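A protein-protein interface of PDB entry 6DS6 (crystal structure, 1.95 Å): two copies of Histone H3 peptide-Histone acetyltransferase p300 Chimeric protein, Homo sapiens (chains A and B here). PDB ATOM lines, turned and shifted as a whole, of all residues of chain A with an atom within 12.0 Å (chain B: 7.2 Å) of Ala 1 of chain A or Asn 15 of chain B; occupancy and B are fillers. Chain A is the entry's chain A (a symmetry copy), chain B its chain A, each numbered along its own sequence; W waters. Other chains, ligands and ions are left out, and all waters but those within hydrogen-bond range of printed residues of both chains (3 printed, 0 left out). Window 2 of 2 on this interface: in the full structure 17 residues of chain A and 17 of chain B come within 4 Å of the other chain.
O of Ala 1 of chain A touches O of Val 11 of chain B, 3.9 Å away.
Tyr 12 of chain B touches Ala 1 of chain A (CA to O, 3.1 Å).
Asp 32 of chain B touches Ala 1 of chain A (OD1 to CA, 3.3 Å).
Arg 2 of chain A touches Val 11 of chain B (CA to O, 3.4 Å).
Tyr 12 of chain B touches Arg 2 of chain A.
Gln 5 of chain A touches Val 11 of chain B (CB to CG1, 3.7 Å).
The side-chain carboxylate (OD1) of Asp 34 of chain B is in salt-bridge range of the guanidinium group (NH1) of Arg 24 of chain B (2.9 Å).
The backbone carbonyl oxygen of Asp 32 of chain B sits at hydrogen-bond distance from the side-chain amide nitrogen of Asn 15 of chain B, at 3.2 Å.
O of Asn 15 of chain B is in hydrogen-bond range of NZ of Lys 18 of chain B.
O of Tyr 12 of chain B is in hydrogen-bond range of N of Val 21 of chain B (3.0 Å).
The backbone NH (N) of Asn 15 of chain B sits at hydrogen-bond distance from the backbone carbonyl oxygen (O) of Asp 34 of chain B, at 2.8 Å.
The side-chain carboxylate (OD1) of Asp 34 of chain B sits at hydrogen-bond distance from a ring nitrogen (ND1) of His 26 of chain B.
No position is printed for both chains.
Ala 1 of chain A touches just these residues of chain B: Val 11, Tyr 12, Thr 13, Asn 15, Asp 32 and Asp 34.
Asn 15 of chain B touches one residue of chain A.
Tyr 12 of chain B touches two residues of chain A.
Of chain A, only Ala 1 comes within 4 Å of Thr 13 of chain B.
No residue of chain A comes within 4 Å of Cys 17 of chain B.
No residue of chain A comes within 4 Å of Lys 18 of chain B.
Of the printed residues of chain A, Asp 32 of chain B touches Ala 1 (3.3 Å) and Arg 2 (2.9 Å).
Asp 34 of chain B touches one residue of chain A.
Leu 35 of chain B touches none of the printed residues of chain A.
Printed residues of chain B within 4 Å of Arg 2 of chain A: Val 11, Tyr 12 and Asp 32.
Printed residues of chain A within 4 Å of Val 11 of chain B: Ala 1, Arg 2, Thr 3 and Gln 5.
Printed residues of chain B within 4 Å of Thr 3 of chain A: Val 11.
Of the printed residues of chain B, Gln 5 of chain A touches Val 11.
The nearest printed residue of chain A that does not touch Val 11 of chain B is Lys 4 of chain A (4.6 Å).
NH1 of Arg 2 of chain A lies within salt-bridge range of OD1 of Asp 32 of chain B.
The side-chain carboxylate (OD2) of Asp 34 of chain B sits at hydrogen-bond distance from the backbone NH (N) of Ala 1 of chain A (2.9 Å).
The backbone NH of Val 11 of chain B is in hydrogen-bond range of the backbone carbonyl oxygen of Thr 3 of chain A.
The backbone carbonyl oxygen of Thr 13 of chain B lies within hydrogen-bond range of the backbone NH of Ala 1 of chain A (2.8 Å).
The side-chain amide oxygen of Asn 15 of chain B sits at hydrogen-bond distance from the backbone NH of Ala 1 of chain A (2.6 Å).
Hydrophobic or aromatic side chains of chain B within 4 Å of the printed part of chain A: Val 11 and Tyr 12.
Along chain B the printed residues that touch a printed residue of chain A span positions 11 to 34.
Hydrophobic or aromatic side chains of chain A within 4 Å of the printed part of chain B: Ala 1.
Among the printed residues, 11 pairs touch across the chains.
Water W2 lies within hydrogen-bond range of O of Arg 2 of chain A (2.5 Å) and OD2 of Asp 32 of chain B (2.6 Å).
Water W1 bridges the backbone carbonyl oxygen (O) of Val 11 of chain B and the side-chain hydroxyl (OG1) of Thr 3 of chain A.
Water W3 lies within hydrogen-bond range of OD2 of Asp 34 of chain B, OD1 of Asp 32 of chain B and NH1 of Arg 2 of chain A.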
ATOM      1  N   ALA A   1     -19.757  16.974 -16.938  1.00  0.00           N
ATOM      2  CA  ALA A   1     -20.558  17.464 -18.071  1.00  0.00           C
ATOM      3  C   ALA A   1     -20.665  16.386 -19.157  1.00  0.00           C
ATOM      4  O   ALA A   1     -19.718  15.630 -19.358  1.00  0.00           O
ATOM      5  CB  ALA A   1     -19.938  18.755 -18.648  1.00  0.00           C
ATOM      6  N   ARG A   2     -21.808  16.316 -19.844  1.00  0.00           N
ATOM      7  CA  ARG A   2     -22.023  15.332 -20.902  1.00  0.00           C
ATOM      8  C   ARG A   2     -22.446  16.025 -22.190  1.00  0.00           C
ATOM      9  O   ARG A   2     -23.183  17.018 -22.159  1.00  0.00           O
ATOM     10  CB  ARG A   2     -23.082  14.288 -20.499  1.00  0.00           C
ATOM     11  CG  ARG A   2     -24.492  14.842 -20.297  1.00  0.00           C
ATOM     12  CD  ARG A   2     -25.446  13.762 -19.782  1.00  0.00           C
ATOM     13  NE  ARG A   2     -26.823  14.241 -19.640  1.00  0.00           N
ATOM     14  CZ  ARG A   2     -27.258  15.021 -18.653  1.00  0.00           C
ATOM     15  NH1 ARG A   2     -26.427  15.431 -17.703  1.00  0.00           N
ATOM     16  NH2 ARG A   2     -28.530  15.394 -18.617  1.00  0.00           N
ATOM     17  N   THR A   3     -21.953  15.508 -23.321  1.00  0.00           N
ATOM     18  CA  THR A   3     -22.417  15.903 -24.643  1.00  0.00           C
ATOM     19  C   THR A   3     -22.564  14.654 -25.512  1.00  0.00           C
ATOM     20  O   THR A   3     -22.088  13.567 -25.170  1.00  0.00           O
ATOM     21  CB  THR A   3     -21.466  16.883 -25.333  1.00  0.00           C
ATOM     22  OG1 THR A   3     -20.210  16.239 -25.545  1.00  0.00           O
ATOM     23  CG2 THR A   3     -21.267  18.176 -24.501  1.00  0.00           C
ATOM     24  N   LYS A   4     -23.224  14.815 -26.648  1.00  0.00           N
ATOM     25  CA  LYS A   4     -23.386  13.719 -27.596  1.00  0.00           C
ATOM     26  C   LYS A   4     -22.187  13.670 -28.533  1.00  0.00           C
ATOM     27  O   LYS A   4     -21.648  14.704 -28.930  1.00  0.00           O
ATOM     28  CB  LYS A   4     -24.674  13.869 -28.409  1.00  0.00           C
ATOM     29  CG  LYS A   4     -25.960  13.754 -27.613  1.00  0.00           C
ATOM     30  CD  LYS A   4     -26.213  12.334 -27.187  1.00  0.00           C
ATOM     31  CE  LYS A   4     -27.658  12.113 -26.762  1.00  0.00           C
ATOM     32  NZ  LYS A   4     -28.637  12.002 -27.877  1.00  0.00           N
ATOM     33  N   GLN A   5     -21.755  12.461 -28.864  1.00  0.00           N
ATOM     34  CA  GLN A   5     -20.800  12.250 -29.937  1.00  0.00           C
ATOM     35  C   GLN A   5     -21.428  11.292 -30.939  1.00  0.00           C
ATOM     36  O   GLN A   5     -21.985  10.259 -30.552  1.00  0.00           O
ATOM     37  CB  GLN A   5     -19.483  11.681 -29.426  1.00  0.00           C
ATOM     38  CG  GLN A   5     -18.556  11.287 -30.546  1.00  0.00           C
ATOM     39  CD  GLN A   5     -17.286  10.631 -30.056  1.00  0.00           C
ATOM     40  OE1 GLN A   5     -17.173   9.406 -30.023  1.00  0.00           O
ATOM     41  NE2 GLN A   5     -16.314  11.439 -29.698  1.00  0.00           N
ATOM     42  N   VAL B  11     -20.415  11.385 -24.092  1.00  0.00           N
ATOM     43  CA  VAL B  11     -19.016  11.558 -23.736  1.00  0.00           C
ATOM     44  C   VAL B  11     -18.980  12.564 -22.585  1.00  0.00           C
ATOM     45  O   VAL B  11     -19.687  13.577 -22.623  1.00  0.00           O
ATOM     46  CB  VAL B  11     -18.180  12.035 -24.937  1.00  0.00           C
ATOM     47  CG1 VAL B  11     -18.117  10.935 -26.058  1.00  0.00           C
ATOM     48  CG2 VAL B  11     -18.789  13.278 -25.518  1.00  0.00           C
ATOM     49  N   TYR B  12     -18.204  12.260 -21.548  1.00  0.00           N
ATOM     50  CA  TYR B  12     -18.207  13.039 -20.309  1.00  0.00           C
ATOM     51  C   TYR B  12     -16.869  13.732 -20.083  1.00  0.00           C
ATOM     52  O   TYR B  12     -15.810  13.184 -20.406  1.00  0.00           O
ATOM     53  CB  TYR B  12     -18.526  12.147 -19.092  1.00  0.00           C
ATOM     54  CG  TYR B  12     -19.894  11.505 -19.149  1.00  0.00           C
ATOM     55  CD1 TYR B  12     -20.980  12.075 -18.508  1.00  0.00           C
ATOM     56  CD2 TYR B  12     -20.101  10.330 -19.871  1.00  0.00           C
ATOM     57  CE1 TYR B  12     -22.231  11.490 -18.567  1.00  0.00           C
ATOM     58  CE2 TYR B  12     -21.344   9.741 -19.935  1.00  0.00           C
ATOM     59  CZ  TYR B  12     -22.408  10.328 -19.290  1.00  0.00           C
ATOM     60  OH  TYR B  12     -23.648   9.741 -19.357  1.00  0.00           O
ATOM     61  N   THR B  13     -16.926  14.942 -19.522  1.00  0.00           N
ATOM     62  CA  THR B  13     -15.756  15.668 -19.050  1.00  0.00           C
ATOM     63  C   THR B  13     -15.937  16.018 -17.577  1.00  0.00           C
ATOM     64  O   THR B  13     -17.063  16.098 -17.071  1.00  0.00           O
ATOM     65  CB  THR B  13     -15.525  16.964 -19.839  1.00  0.00           C
ATOM     66  OG1 THR B  13     -16.701  17.783 -19.761  1.00  0.00           O
ATOM     67  CG2 THR B  13     -15.199  16.670 -21.310  1.00  0.00           C
ATOM     68  N   CYS B  14     -14.817  16.239 -16.887  1.00  0.00           N
ATOM     69  CA  CYS B  14     -14.877  16.716 -15.508  1.00  0.00           C
ATOM     70  C   CYS B  14     -15.191  18.202 -15.505  1.00  0.00           C
ATOM     71  O   CYS B  14     -14.506  18.984 -16.165  1.00  0.00           O
ATOM     72  CB  CYS B  14     -13.563  16.464 -14.768  1.00  0.00           C
ATOM     73  SG  CYS B  14     -13.503  17.355 -13.166  1.00  0.00           S
ATOM     74  N   ASN B  15     -16.234  18.597 -14.773  1.00  0.00           N
ATOM     75  CA  ASN B  15     -16.609  20.003 -14.769  1.00  0.00           C
ATOM     76  C   ASN B  15     -15.508  20.888 -14.191  1.00  0.00           C
ATOM     77  O   ASN B  15     -15.499  22.094 -14.461  1.00  0.00           O
ATOM     78  CB  ASN B  15     -17.892  20.222 -13.966  1.00  0.00           C
ATOM     79  CG  ASN B  15     -19.127  19.793 -14.697  1.00  0.00           C
ATOM     80  OD1 ASN B  15     -19.305  18.616 -15.018  1.00  0.00           O
ATOM     81  ND2 ASN B  15     -20.022  20.739 -14.933  1.00  0.00           N
ATOM     82  N   GLU B  16     -14.583  20.315 -13.413  1.00  0.00           N
ATOM     83  CA  GLU B  16     -13.515  21.076 -12.761  1.00  0.00           C
ATOM     84  C   GLU B  16     -12.268  21.195 -13.632  1.00  0.00           C
ATOM     85  O   GLU B  16     -11.875  22.303 -14.006  1.00  0.00           O
ATOM     86  CB  GLU B  16     -13.149  20.449 -11.412  1.00  0.00           C
ATOM     87  CG  GLU B  16     -14.124  20.805 -10.322  1.00  0.00           C
ATOM     88  CD  GLU B  16     -14.328  22.297 -10.197  1.00  0.00           C
ATOM     89  OE1 GLU B  16     -13.315  23.009  -9.998  1.00  0.00           O
ATOM     90  OE2 GLU B  16     -15.495  22.749 -10.286  1.00  0.00           O
ATOM     91  N   CYS B  17     -11.632  20.075 -13.957  1.00  0.00           N
ATOM     92  CA  CYS B  17     -10.392  20.146 -14.717  1.00  0.00           C
ATOM     93  C   CYS B  17     -10.608  20.059 -16.224  1.00  0.00           C
ATOM     94  O   CYS B  17      -9.635  20.157 -16.976  1.00  0.00           O
ATOM     95  CB  CYS B  17      -9.409  19.060 -14.252  1.00  0.00           C
ATOM     96  SG  CYS B  17      -9.864  17.325 -14.515  1.00  0.00           S
ATOM     97  N   LYS B  18     -11.854  19.893 -16.677  1.00  0.00           N
ATOM     98  CA  LYS B  18     -12.258  19.849 -18.083  1.00  0.00           C
ATOM     99  C   LYS B  18     -11.696  18.655 -18.835  1.00  0.00           C
ATOM    100  O   LYS B  18     -11.848  18.581 -20.061  1.00  0.00           O
ATOM    101  CB  LYS B  18     -11.887  21.139 -18.831  1.00  0.00           C
ATOM    102  CG  LYS B  18     -12.169  22.423 -18.061  1.00  0.00           C
ATOM    103  CD  LYS B  18     -13.634  22.559 -17.710  1.00  0.00           C
ATOM    104  CE  LYS B  18     -13.963  23.951 -17.182  1.00  0.00           C
ATOM    105  NZ  LYS B  18     -15.415  24.105 -16.866  1.00  0.00           N
ATOM    106  N   HIS B  19     -11.059  17.712 -18.147  1.00  0.00           N
ATOM    107  CA  HIS B  19     -10.544  16.532 -18.820  1.00  0.00           C
ATOM    108  C   HIS B  19     -11.651  15.529 -19.121  1.00  0.00           C
ATOM    109  O   HIS B  19     -12.701  15.503 -18.468  1.00  0.00           O
ATOM    110  CB  HIS B  19      -9.468  15.848 -17.979  1.00  0.00           C
ATOM    111  CG  HIS B  19      -8.187  16.617 -17.891  1.00  0.00           C
ATOM    112  ND1 HIS B  19      -8.149  17.986 -17.726  1.00  0.00           N
ATOM    113  CD2 HIS B  19      -6.898  16.206 -17.931  1.00  0.00           C
ATOM    114  CE1 HIS B  19      -6.892  18.385 -17.674  1.00  0.00           C
ATOM    115  NE2 HIS B  19      -6.111  17.325 -17.795  1.00  0.00           N
ATOM    116  N   VAL B  21     -13.443  12.073 -18.938  1.00  0.00           N
ATOM    117  CA  VAL B  21     -13.598  11.092 -17.869  1.00  0.00           C
ATOM    118  C   VAL B  21     -14.459   9.947 -18.369  1.00  0.00           C
ATOM    119  O   VAL B  21     -15.419  10.159 -19.116  1.00  0.00           O
ATOM    120  CB  VAL B  21     -14.220  11.714 -16.598  1.00  0.00           C
ATOM    121  CG1 VAL B  21     -13.197  12.554 -15.894  1.00  0.00           C
ATOM    122  CG2 VAL B  21     -15.444  12.573 -16.931  1.00  0.00           C
ATOM    123  N   ARG B  24     -16.339   8.398 -13.235  1.00  0.00           N
ATOM    124  CA  ARG B  24     -16.719   9.756 -12.892  1.00  0.00           C
ATOM    125  C   ARG B  24     -17.651   9.742 -11.690  1.00  0.00           C
ATOM    126  O   ARG B  24     -18.468   8.828 -11.528  1.00  0.00           O
ATOM    127  CB  ARG B  24     -17.407  10.452 -14.069  1.00  0.00           C
ATOM    128  CG  ARG B  24     -18.658   9.714 -14.539  1.00  0.00           C
ATOM    129  CD  ARG B  24     -19.237  10.306 -15.818  1.00  0.00           C
ATOM    130  NE  ARG B  24     -20.223   9.383 -16.364  1.00  0.00           N
ATOM    131  CZ  ARG B  24     -21.520   9.445 -16.086  1.00  0.00           C
ATOM    132  NH1 ARG B  24     -21.979  10.398 -15.286  1.00  0.00           N
ATOM    133  NH2 ARG B  24     -22.358   8.562 -16.610  1.00  0.00           N
ATOM    134  N   TRP B  25     -17.509  10.755 -10.851  1.00  0.00           N
ATOM    135  CA  TRP B  25     -18.465  11.011  -9.791  1.00  0.00           C
ATOM    136  C   TRP B  25     -19.541  11.912 -10.371  1.00  0.00           C
ATOM    137  O   TRP B  25     -19.242  13.011 -10.852  1.00  0.00           O
ATOM    138  CB  TRP B  25     -17.789  11.662  -8.574  1.00  0.00           C
ATOM    139  CG  TRP B  25     -17.065  10.680  -7.709  1.00  0.00           C
ATOM    140  CD1 TRP B  25     -15.765  10.260  -7.843  1.00  0.00           C
ATOM    141  CD2 TRP B  25     -17.602   9.979  -6.584  1.00  0.00           C
ATOM    142  NE1 TRP B  25     -15.466   9.356  -6.859  1.00  0.00           N
ATOM    143  CE2 TRP B  25     -16.572   9.171  -6.066  1.00  0.00           C
ATOM    144  CE3 TRP B  25     -18.844   9.985  -5.939  1.00  0.00           C
ATOM    145  CZ2 TRP B  25     -16.748   8.366  -4.939  1.00  0.00           C
ATOM    146  CZ3 TRP B  25     -19.020   9.181  -4.812  1.00  0.00           C
ATOM    147  CH2 TRP B  25     -17.978   8.387  -4.328  1.00  0.00           C
ATOM    148  N   HIS B  26     -20.785  11.442 -10.358  1.00  0.00           N
ATOM    149  CA  HIS B  26     -21.884  12.169 -10.971  1.00  0.00           C
ATOM    150  C   HIS B  26     -22.770  12.758  -9.880  1.00  0.00           C
ATOM    151  O   HIS B  26     -23.170  12.049  -8.950  1.00  0.00           O
ATOM    152  CB  HIS B  26     -22.695  11.249 -11.890  1.00  0.00           C
ATOM    153  CG  HIS B  26     -23.838  11.934 -12.564  1.00  0.00           C
ATOM    154  ND1 HIS B  26     -23.661  12.864 -13.565  1.00  0.00           N
ATOM    155  CD2 HIS B  26     -25.174  11.832 -12.374  1.00  0.00           C
ATOM    156  CE1 HIS B  26     -24.841  13.296 -13.974  1.00  0.00           C
ATOM    157  NE2 HIS B  26     -25.776  12.690 -13.263  1.00  0.00           N
ATOM    158  N   CYS B  30     -27.319  18.371  -9.379  1.00  0.00           N
ATOM    159  CA  CYS B  30     -27.096  19.174 -10.571  1.00  0.00           C
ATOM    160  C   CYS B  30     -27.583  18.411 -11.789  1.00  0.00           C
ATOM    161  O   CYS B  30     -27.729  17.186 -11.770  1.00  0.00           O
ATOM    162  CB  CYS B  30     -25.617  19.535 -10.714  1.00  0.00           C
ATOM    163  SG  CYS B  30     -24.991  20.668  -9.387  1.00  0.00           S
ATOM    164  N   ASP B  32     -25.975  18.524 -14.769  1.00  0.00           N
ATOM    165  CA  ASP B  32     -24.889  18.183 -15.681  1.00  0.00           C
ATOM    166  C   ASP B  32     -23.513  18.341 -15.049  1.00  0.00           C
ATOM    167  O   ASP B  32     -22.612  18.933 -15.646  1.00  0.00           O
ATOM    168  CB  ASP B  32     -24.999  19.051 -16.939  1.00  0.00           C
ATOM    169  CG  ASP B  32     -24.110  18.569 -18.061  1.00  0.00           C
ATOM    170  OD1 ASP B  32     -23.894  17.351 -18.145  1.00  0.00           O
ATOM    171  OD2 ASP B  32     -23.623  19.404 -18.851  1.00  0.00           O
ATOM    172  N   TYR B  33     -23.316  17.801 -13.849  1.00  0.00           N
ATOM    173  CA  TYR B  33     -22.074  18.009 -13.109  1.00  0.00           C
ATOM    174  C   TYR B  33     -21.389  16.674 -12.848  1.00  0.00           C
ATOM    175  O   TYR B  33     -21.964  15.790 -12.205  1.00  0.00           O
ATOM    176  CB  TYR B  33     -22.339  18.755 -11.793  1.00  0.00           C
ATOM    177  CG  TYR B  33     -21.085  19.290 -11.135  1.00  0.00           C
ATOM    178  CD1 TYR B  33     -20.594  20.563 -11.438  1.00  0.00           C
ATOM    179  CD2 TYR B  33     -20.385  18.518 -10.214  1.00  0.00           C
ATOM    180  CE1 TYR B  33     -19.444  21.044 -10.841  1.00  0.00           C
ATOM    181  CE2 TYR B  33     -19.227  18.987  -9.608  1.00  0.00           C
ATOM    182  CZ  TYR B  33     -18.767  20.252  -9.925  1.00  0.00           C
ATOM    183  OH  TYR B  33     -17.625  20.709  -9.325  1.00  0.00           O
ATOM    184  N   ASP B  34     -20.152  16.538 -13.329  1.00  0.00           N
ATOM    185  CA  ASP B  34     -19.341  15.352 -13.103  1.00  0.00           C
ATOM    186  C   ASP B  34     -17.943  15.762 -12.643  1.00  0.00           C
ATOM    187  O   ASP B  34     -17.443  16.832 -12.999  1.00  0.00           O
ATOM    188  CB  ASP B  34     -19.254  14.495 -14.383  1.00  0.00           C
ATOM    189  CG  ASP B  34     -20.618  14.068 -14.890  1.00  0.00           C
ATOM    190  OD1 ASP B  34     -21.132  13.040 -14.405  1.00  0.00           O
ATOM    191  OD2 ASP B  34     -21.200  14.782 -15.741  1.00  0.00           O
ATOM    192  N   LEU B  35     -17.308  14.891 -11.855  1.00  0.00           N
ATOM    193  CA  LEU B  35     -15.931  15.070 -11.425  1.00  0.00           C
ATOM    194  C   LEU B  35     -15.121  13.824 -11.730  1.00  0.00           C
ATOM    195  O   LEU B  35     -15.588  12.700 -11.522  1.00  0.00           O
ATOM    196  CB  LEU B  35     -15.837  15.355  -9.916  1.00  0.00           C
ATOM    197  CG  LEU B  35     -16.421  16.657  -9.385  1.00  0.00           C
ATOM    198  CD1 LEU B  35     -16.205  16.744  -7.883  1.00  0.00           C
ATOM    199  CD2 LEU B  35     -15.754  17.818 -10.089  1.00  0.00           C
ATOM    200  N   CYS B  36     -13.888  14.030 -12.194  1.00  0.00           N
ATOM    201  CA  CYS B  36     -12.909  12.957 -12.192  1.00  0.00           C
ATOM    202  C   CYS B  36     -12.573  12.566 -10.755  1.00  0.00           C
ATOM    203  O   CYS B  36     -12.872  13.286  -9.795  1.00  0.00           O
ATOM    204  CB  CYS B  36     -11.640  13.367 -12.954  1.00  0.00           C
ATOM    205  SG  CYS B  36     -10.630  14.697 -12.207  1.00  0.00           S
ATOM    206  N   CYS B  39     -10.291  15.140  -8.875  1.00  0.00           N
ATOM    207  CA  CYS B  39     -11.024  16.324  -8.439  1.00  0.00           C
ATOM    208  C   CYS B  39     -12.073  16.005  -7.375  1.00  0.00           C
ATOM    209  O   CYS B  39     -12.334  16.845  -6.498  1.00  0.00           O
ATOM    210  CB  CYS B  39     -11.694  16.998  -9.632  1.00  0.00           C
ATOM    211  SG  CYS B  39     -10.566  17.905 -10.712  1.00  0.00           S
HETATM  212  O   HOH W   1     -18.533  15.904 -23.131  1.00  0.00           O
HETATM  213  O   HOH W   2     -22.860  19.382 -21.339  1.00  0.00           O
HETATM  214  O   HOH W   3     -23.647  14.915 -16.841  1.00  0.00           O
